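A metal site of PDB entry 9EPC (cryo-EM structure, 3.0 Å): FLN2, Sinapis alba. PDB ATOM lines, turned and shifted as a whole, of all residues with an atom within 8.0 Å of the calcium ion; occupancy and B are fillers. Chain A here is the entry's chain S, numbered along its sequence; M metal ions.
O of Asp 376 lies close to OG1 of Thr 346. O of Pro 246 sits close to OD1 of Asn 378 (3.2 Å). The side-chain hydroxyl (OG1) of Thr 455 sits at hydrogen-bond distance from the side-chain carboxylate (OE2) of Glu 405, at 2.5 Å. N of Leu 377 sits at hydrogen-bond distance from O of Glu 405, at 3.0 Å. The backbone NH of Glu 405 lies within hydrogen-bond range of the backbone carbonyl oxygen of Tyr 375, at 3.1 Å. OE2 of Glu 410 sits close to N of Asn 378, 3.3 Å away. The side-chain carboxylate (OD2) of Asp 376 is in hydrogen-bond range of the side-chain hydroxyl (OH) of Tyr 344, at 3.0 Å.
O of Pro 246 touches the calcium ion, 3.2 Å away. Of the 28 residues printed, 4 come within 4 Å of the calcium ion. Along chain A the residues within 4 Å of the calcium ion span positions 246 to 405. The nearest printed residue that does not touch the calcium ion is Thr 407 (4.01 Å).
OD1 of Asp 376 is bound to the calcium ion (2.3 Å). The calcium ion is bound by the side-chain amide oxygen (OD1) of Asn 378, 2.4 Å away. The calcium ion is bound by OE1 of Glu 405 (2.5 Å). The calcium ion has three donor atoms within binding distance.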
ATOM      1  N   PRO A 215      17.251   3.947 -17.088  1.00  0.00           N
ATOM      2  CA  PRO A 215      18.220   4.374 -16.070  1.00  0.00           C
ATOM      3  C   PRO A 215      18.613   5.829 -16.219  1.00  0.00           C
ATOM      4  O   PRO A 215      18.486   6.605 -15.264  1.00  0.00           O
ATOM      5  CB  PRO A 215      19.408   3.427 -16.294  1.00  0.00           C
ATOM      6  CG  PRO A 215      18.837   2.261 -17.036  1.00  0.00           C
ATOM      7  CD  PRO A 215      17.771   2.832 -17.907  1.00  0.00           C
ATOM      8  N   ALA A 245      18.952   6.489 -24.328  1.00  0.00           N
ATOM      9  CA  ALA A 245      19.094   5.762 -23.084  1.00  0.00           C
ATOM     10  C   ALA A 245      19.884   4.479 -23.300  1.00  0.00           C
ATOM     11  O   ALA A 245      19.812   3.865 -24.370  1.00  0.00           O
ATOM     12  CB  ALA A 245      17.717   5.428 -22.509  1.00  0.00           C
ATOM     13  N   PRO A 246      20.663   4.048 -22.300  1.00  0.00           N
ATOM     14  CA  PRO A 246      21.443   2.816 -22.473  1.00  0.00           C
ATOM     15  C   PRO A 246      20.593   1.568 -22.630  1.00  0.00           C
ATOM     16  O   PRO A 246      21.090   0.566 -23.160  1.00  0.00           O
ATOM     17  CB  PRO A 246      22.283   2.758 -21.185  1.00  0.00           C
ATOM     18  CG  PRO A 246      21.489   3.526 -20.197  1.00  0.00           C
ATOM     19  CD  PRO A 246      20.853   4.645 -20.977  1.00  0.00           C
ATOM     20  N   GLY A 247      19.354   1.596 -22.202  1.00  0.00           N
ATOM     21  CA  GLY A 247      18.490   0.438 -22.272  1.00  0.00           C
ATOM     22  C   GLY A 247      17.407   0.547 -21.207  1.00  0.00           C
ATOM     23  O   GLY A 247      17.033   1.639 -20.799  1.00  0.00           O
ATOM     24  N   GLY A 248      16.923  -0.614 -20.778  1.00  0.00           N
ATOM     25  CA  GLY A 248      15.894  -0.703 -19.766  1.00  0.00           C
ATOM     26  C   GLY A 248      16.337  -1.563 -18.608  1.00  0.00           C
ATOM     27  O   GLY A 248      17.526  -1.727 -18.336  1.00  0.00           O
ATOM     28  N   VAL A 253      15.261  -6.975 -20.833  1.00  0.00           N
ATOM     29  CA  VAL A 253      16.184  -7.788 -21.613  1.00  0.00           C
ATOM     30  C   VAL A 253      15.683  -9.221 -21.705  1.00  0.00           C
ATOM     31  O   VAL A 253      15.762  -9.854 -22.773  1.00  0.00           O
ATOM     32  CB  VAL A 253      17.595  -7.715 -21.012  1.00  0.00           C
ATOM     33  CG1 VAL A 253      18.556  -8.592 -21.797  1.00  0.00           C
ATOM     34  CG2 VAL A 253      18.079  -6.288 -20.995  1.00  0.00           C
ATOM     35  N   TYR A 344      23.123 -12.614 -16.284  1.00  0.00           N
ATOM     36  CA  TYR A 344      22.985 -11.241 -16.744  1.00  0.00           C
ATOM     37  C   TYR A 344      22.513 -10.360 -15.594  1.00  0.00           C
ATOM     38  O   TYR A 344      21.628 -10.756 -14.829  1.00  0.00           O
ATOM     39  CB  TYR A 344      22.004 -11.152 -17.921  1.00  0.00           C
ATOM     40  CG  TYR A 344      21.720  -9.736 -18.354  1.00  0.00           C
ATOM     41  CD1 TYR A 344      22.527  -9.095 -19.273  1.00  0.00           C
ATOM     42  CD2 TYR A 344      20.636  -9.044 -17.836  1.00  0.00           C
ATOM     43  CE1 TYR A 344      22.274  -7.805 -19.672  1.00  0.00           C
ATOM     44  CE2 TYR A 344      20.374  -7.750 -18.237  1.00  0.00           C
ATOM     45  CZ  TYR A 344      21.185  -7.144 -19.150  1.00  0.00           C
ATOM     46  OH  TYR A 344      20.922  -5.849 -19.541  1.00  0.00           O
ATOM     47  N   THR A 346      22.546  -5.814 -14.279  1.00  0.00           N
ATOM     48  CA  THR A 346      22.795  -4.430 -14.622  1.00  0.00           C
ATOM     49  C   THR A 346      23.192  -3.659 -13.365  1.00  0.00           C
ATOM     50  O   THR A 346      23.078  -4.161 -12.245  1.00  0.00           O
ATOM     51  CB  THR A 346      21.576  -3.773 -15.278  1.00  0.00           C
ATOM     52  OG1 THR A 346      21.826  -2.383 -15.488  1.00  0.00           O
ATOM     53  CG2 THR A 346      20.348  -3.946 -14.408  1.00  0.00           C
ATOM     54  N   PHE A 374      27.537 -11.836 -17.767  1.00  0.00           N
ATOM     55  CA  PHE A 374      27.292 -10.705 -18.656  1.00  0.00           C
ATOM     56  C   PHE A 374      26.890  -9.503 -17.816  1.00  0.00           C
ATOM     57  O   PHE A 374      25.983  -9.605 -16.985  1.00  0.00           O
ATOM     58  CB  PHE A 374      26.207 -11.040 -19.670  1.00  0.00           C
ATOM     59  CG  PHE A 374      26.178 -10.121 -20.857  1.00  0.00           C
ATOM     60  CD1 PHE A 374      25.668  -8.838 -20.740  1.00  0.00           C
ATOM     61  CD2 PHE A 374      26.651 -10.534 -22.084  1.00  0.00           C
ATOM     62  CE1 PHE A 374      25.636  -7.992 -21.835  1.00  0.00           C
ATOM     63  CE2 PHE A 374      26.614  -9.697 -23.178  1.00  0.00           C
ATOM     64  CZ  PHE A 374      26.111  -8.417 -23.049  1.00  0.00           C
ATOM     65  N   TYR A 375      27.564  -8.373 -18.028  1.00  0.00           N
ATOM     66  CA  TYR A 375      27.329  -7.167 -17.248  1.00  0.00           C
ATOM     67  C   TYR A 375      27.018  -6.017 -18.195  1.00  0.00           C
ATOM     68  O   TYR A 375      27.933  -5.346 -18.694  1.00  0.00           O
ATOM     69  CB  TYR A 375      28.531  -6.853 -16.362  1.00  0.00           C
ATOM     70  CG  TYR A 375      28.355  -5.618 -15.492  1.00  0.00           C
ATOM     71  CD1 TYR A 375      27.098  -5.148 -15.162  1.00  0.00           C
ATOM     72  CD2 TYR A 375      29.458  -4.934 -15.008  1.00  0.00           C
ATOM     73  CE1 TYR A 375      26.940  -4.038 -14.373  1.00  0.00           C
ATOM     74  CE2 TYR A 375      29.307  -3.816 -14.230  1.00  0.00           C
ATOM     75  CZ  TYR A 375      28.043  -3.365 -13.909  1.00  0.00           C
ATOM     76  OH  TYR A 375      27.887  -2.256 -13.130  1.00  0.00           O
ATOM     77  N   ASP A 376      25.732  -5.781 -18.444  1.00  0.00           N
ATOM     78  CA  ASP A 376      25.310  -4.564 -19.114  1.00  0.00           C
ATOM     79  C   ASP A 376      25.354  -3.434 -18.102  1.00  0.00           C
ATOM     80  O   ASP A 376      24.706  -3.501 -17.059  1.00  0.00           O
ATOM     81  CB  ASP A 376      23.900  -4.737 -19.691  1.00  0.00           C
ATOM     82  CG  ASP A 376      23.438  -3.527 -20.481  1.00  0.00           C
ATOM     83  OD1 ASP A 376      24.194  -2.546 -20.593  1.00  0.00           O
ATOM     84  OD2 ASP A 376      22.301  -3.557 -21.002  1.00  0.00           O
ATOM     85  N   LEU A 377      26.125  -2.390 -18.406  1.00  0.00           N
ATOM     86  CA  LEU A 377      26.307  -1.299 -17.464  1.00  0.00           C
ATOM     87  C   LEU A 377      24.991  -0.589 -17.201  1.00  0.00           C
ATOM     88  O   LEU A 377      24.460  -0.656 -16.082  1.00  0.00           O
ATOM     89  CB  LEU A 377      27.358  -0.316 -17.981  1.00  0.00           C
ATOM     90  CG  LEU A 377      27.923   0.619 -16.920  1.00  0.00           C
ATOM     91  CD1 LEU A 377      28.624  -0.184 -15.842  1.00  0.00           C
ATOM     92  CD2 LEU A 377      28.885   1.621 -17.539  1.00  0.00           C
ATOM     93  N   ASN A 378      24.432   0.067 -18.219  1.00  0.00           N
ATOM     94  CA  ASN A 378      23.197   0.842 -18.093  1.00  0.00           C
ATOM     95  C   ASN A 378      23.253   1.751 -16.852  1.00  0.00           C
ATOM     96  O   ASN A 378      22.492   1.592 -15.900  1.00  0.00           O
ATOM     97  CB  ASN A 378      21.973  -0.073 -18.043  1.00  0.00           C
ATOM     98  CG  ASN A 378      21.774  -0.833 -19.333  1.00  0.00           C
ATOM     99  OD1 ASN A 378      22.261  -0.428 -20.395  1.00  0.00           O
ATOM    100  ND2 ASN A 378      21.054  -1.946 -19.257  1.00  0.00           N
ATOM    101  N   LEU A 379      24.187   2.690 -16.891  1.00  0.00           N
ATOM    102  CA  LEU A 379      24.509   3.473 -15.713  1.00  0.00           C
ATOM    103  C   LEU A 379      23.281   4.258 -15.257  1.00  0.00           C
ATOM    104  O   LEU A 379      22.684   4.987 -16.047  1.00  0.00           O
ATOM    105  CB  LEU A 379      25.655   4.439 -16.023  1.00  0.00           C
ATOM    106  CG  LEU A 379      26.633   4.698 -14.876  1.00  0.00           C
ATOM    107  CD1 LEU A 379      27.264   3.388 -14.429  1.00  0.00           C
ATOM    108  CD2 LEU A 379      27.696   5.678 -15.317  1.00  0.00           C
ATOM    109  N   ILE A 404      31.215  -7.602 -20.908  1.00  0.00           N
ATOM    110  CA  ILE A 404      30.698  -6.322 -20.432  1.00  0.00           C
ATOM    111  C   ILE A 404      30.224  -5.527 -21.639  1.00  0.00           C
ATOM    112  O   ILE A 404      30.957  -5.389 -22.614  1.00  0.00           O
ATOM    113  CB  ILE A 404      31.768  -5.542 -19.650  1.00  0.00           C
ATOM    114  CG1 ILE A 404      32.281  -6.370 -18.481  1.00  0.00           C
ATOM    115  CG2 ILE A 404      31.181  -4.227 -19.151  1.00  0.00           C
ATOM    116  CD1 ILE A 404      33.357  -5.681 -17.674  1.00  0.00           C
ATOM    117  N   GLU A 405      29.007  -5.021 -21.563  1.00  0.00           N
ATOM    118  CA  GLU A 405      28.433  -4.179 -22.611  1.00  0.00           C
ATOM    119  C   GLU A 405      28.208  -2.785 -22.031  1.00  0.00           C
ATOM    120  O   GLU A 405      27.446  -2.618 -21.075  1.00  0.00           O
ATOM    121  CB  GLU A 405      27.123  -4.772 -23.139  1.00  0.00           C
ATOM    122  CG  GLU A 405      26.614  -4.130 -24.414  1.00  0.00           C
ATOM    123  CD  GLU A 405      25.783  -2.892 -24.169  1.00  0.00           C
ATOM    124  OE1 GLU A 405      25.374  -2.671 -23.016  1.00  0.00           O
ATOM    125  OE2 GLU A 405      25.530  -2.142 -25.130  1.00  0.00           O
ATOM    126  N   VAL A 406      28.875  -1.801 -22.614  1.00  0.00           N
ATOM    127  CA  VAL A 406      28.738  -0.414 -22.201  1.00  0.00           C
ATOM    128  C   VAL A 406      28.445   0.435 -23.431  1.00  0.00           C
ATOM    129  O   VAL A 406      28.840   0.088 -24.548  1.00  0.00           O
ATOM    130  CB  VAL A 406      30.005   0.108 -21.476  1.00  0.00           C
ATOM    131  CG1 VAL A 406      30.247  -0.680 -20.203  1.00  0.00           C
ATOM    132  CG2 VAL A 406      31.214   0.008 -22.394  1.00  0.00           C
ATOM    133  N   THR A 407      27.749   1.536 -23.212  1.00  0.00           N
ATOM    134  CA  THR A 407      27.517   2.460 -24.317  1.00  0.00           C
ATOM    135  C   THR A 407      28.776   3.281 -24.583  1.00  0.00           C
ATOM    136  O   THR A 407      29.709   3.313 -23.773  1.00  0.00           O
ATOM    137  CB  THR A 407      26.341   3.381 -24.014  1.00  0.00           C
ATOM    138  OG1 THR A 407      26.735   4.344 -23.032  1.00  0.00           O
ATOM    139  CG2 THR A 407      25.163   2.586 -23.488  1.00  0.00           C
ATOM    140  N   LYS A 408      28.795   3.942 -25.734  1.00  0.00           N
ATOM    141  CA  LYS A 408      29.922   4.816 -26.056  1.00  0.00           C
ATOM    142  C   LYS A 408      30.027   5.948 -25.053  1.00  0.00           C
ATOM    143  O   LYS A 408      31.130   6.316 -24.637  1.00  0.00           O
ATOM    144  CB  LYS A 408      29.771   5.361 -27.471  1.00  0.00           C
ATOM    145  CG  LYS A 408      30.887   6.294 -27.896  1.00  0.00           C
ATOM    146  CD  LYS A 408      30.731   6.716 -29.346  1.00  0.00           C
ATOM    147  CE  LYS A 408      31.706   7.811 -29.719  1.00  0.00           C
ATOM    148  NZ  LYS A 408      31.447   9.072 -28.962  1.00  0.00           N
ATOM    149  N   GLU A 410      28.986   5.808 -21.925  1.00  0.00           N
ATOM    150  CA  GLU A 410      29.442   5.214 -20.668  1.00  0.00           C
ATOM    151  C   GLU A 410      30.943   4.936 -20.699  1.00  0.00           C
ATOM    152  O   GLU A 410      31.637   5.142 -19.704  1.00  0.00           O
ATOM    153  CB  GLU A 410      28.663   3.938 -20.375  1.00  0.00           C
ATOM    154  CG  GLU A 410      27.232   4.187 -19.935  1.00  0.00           C
ATOM    155  CD  GLU A 410      26.370   2.937 -20.011  1.00  0.00           C
ATOM    156  OE1 GLU A 410      26.823   1.933 -20.591  1.00  0.00           O
ATOM    157  OE2 GLU A 410      25.237   2.971 -19.491  1.00  0.00           O
ATOM    158  N   PHE A 453      31.857  -4.850 -25.167  1.00  0.00           N
ATOM    159  CA  PHE A 453      31.011  -4.309 -26.227  1.00  0.00           C
ATOM    160  C   PHE A 453      30.761  -2.837 -25.961  1.00  0.00           C
ATOM    161  O   PHE A 453      30.253  -2.469 -24.900  1.00  0.00           O
ATOM    162  CB  PHE A 453      29.686  -5.067 -26.322  1.00  0.00           C
ATOM    163  CG  PHE A 453      29.797  -6.395 -26.996  1.00  0.00           C
ATOM    164  CD1 PHE A 453      30.012  -6.470 -28.353  1.00  0.00           C
ATOM    165  CD2 PHE A 453      29.675  -7.571 -26.277  1.00  0.00           C
ATOM    166  CE1 PHE A 453      30.112  -7.702 -28.982  1.00  0.00           C
ATOM    167  CE2 PHE A 453      29.778  -8.793 -26.896  1.00  0.00           C
ATOM    168  CZ  PHE A 453      29.997  -8.859 -28.253  1.00  0.00           C
ATOM    169  N   THR A 455      28.624   0.142 -27.513  1.00  0.00           N
ATOM    170  CA  THR A 455      27.497   0.339 -28.416  1.00  0.00           C
ATOM    171  C   THR A 455      27.145   1.815 -28.490  1.00  0.00           C
ATOM    172  O   THR A 455      26.958   2.467 -27.457  1.00  0.00           O
ATOM    173  CB  THR A 455      26.288  -0.466 -27.966  1.00  0.00           C
ATOM    174  OG1 THR A 455      25.981  -0.154 -26.600  1.00  0.00           O
ATOM    175  CG2 THR A 455      26.569  -1.960 -28.088  1.00  0.00           C
ATOM    176  N   SER A 490      15.994  -0.208 -28.312  1.00  0.00           N
ATOM    177  CA  SER A 490      17.216  -0.586 -29.023  1.00  0.00           C
ATOM    178  C   SER A 490      18.263  -1.121 -28.057  1.00  0.00           C
ATOM    179  O   SER A 490      18.945  -2.106 -28.347  1.00  0.00           O
ATOM    180  CB  SER A 490      17.764   0.606 -29.804  1.00  0.00           C
ATOM    181  OG  SER A 490      16.844   1.043 -30.781  1.00  0.00           O
ATOM    182  N   GLY A 491      18.402  -0.482 -26.895  1.00  0.00           N
ATOM    183  CA  GLY A 491      19.359  -0.959 -25.915  1.00  0.00           C
ATOM    184  C   GLY A 491      19.051  -2.365 -25.437  1.00  0.00           C
ATOM    185  O   GLY A 491      19.936  -3.212 -25.335  1.00  0.00           O
ATOM    186  N   ASP A 492      17.772  -2.625 -25.130  1.00  0.00           N
ATOM    187  CA  ASP A 492      17.378  -3.968 -24.730  1.00  0.00           C
ATOM    188  C   ASP A 492      17.523  -4.952 -25.878  1.00  0.00           C
ATOM    189  O   ASP A 492      17.958  -6.094 -25.670  1.00  0.00           O
ATOM    190  CB  ASP A 492      15.936  -3.957 -24.216  1.00  0.00           C
ATOM    191  CG  ASP A 492      15.773  -3.084 -22.994  1.00  0.00           C
ATOM    192  OD1 ASP A 492      16.769  -2.493 -22.539  1.00  0.00           O
ATOM    193  OD2 ASP A 492      14.626  -2.988 -22.485  1.00  0.00           O
ATOM    194  N   ILE A 494      19.631  -4.788 -28.404  1.00  0.00           N
ATOM    195  CA  ILE A 494      21.036  -5.008 -28.741  1.00  0.00           C
ATOM    196  C   ILE A 494      21.651  -6.031 -27.792  1.00  0.00           C
ATOM    197  O   ILE A 494      22.306  -6.986 -28.225  1.00  0.00           O
ATOM    198  CB  ILE A 494      21.802  -3.678 -28.715  1.00  0.00           C
ATOM    199  CG1 ILE A 494      21.519  -2.881 -29.987  1.00  0.00           C
ATOM    200  CG2 ILE A 494      23.292  -3.933 -28.576  1.00  0.00           C
ATOM    201  CD1 ILE A 494      22.129  -1.508 -29.988  1.00  0.00           C
ATOM    202  N   VAL A 495      21.459  -5.846 -26.488  1.00  0.00           N
ATOM    203  CA  VAL A 495      22.040  -6.797 -25.536  1.00  0.00           C
ATOM    204  C   VAL A 495      21.389  -8.166 -25.677  1.00  0.00           C
ATOM    205  O   VAL A 495      22.052  -9.190 -25.501  1.00  0.00           O
ATOM    206  CB  VAL A 495      21.939  -6.260 -24.098  1.00  0.00           C
ATOM    207  CG1 VAL A 495      22.783  -5.010 -23.953  1.00  0.00           C
ATOM    208  CG2 VAL A 495      20.503  -5.967 -23.727  1.00  0.00           C
ATOM    209  N   LEU A 498      23.129  -9.811 -28.452  1.00  0.00           N
ATOM    210  CA  LEU A 498      24.463 -10.199 -28.026  1.00  0.00           C
ATOM    211  C   LEU A 498      24.419 -11.465 -27.165  1.00  0.00           C
ATOM    212  O   LEU A 498      25.238 -12.369 -27.346  1.00  0.00           O
ATOM    213  CB  LEU A 498      25.115  -9.062 -27.255  1.00  0.00           C
ATOM    214  CG  LEU A 498      25.470  -7.817 -28.071  1.00  0.00           C
ATOM    215  CD1 LEU A 498      25.952  -6.701 -27.176  1.00  0.00           C
ATOM    216  CD2 LEU A 498      26.515  -8.153 -29.112  1.00  0.00           C
HETATM  217 CA    CA M   1      23.724  -0.941 -22.243  1.00  0.00          CA
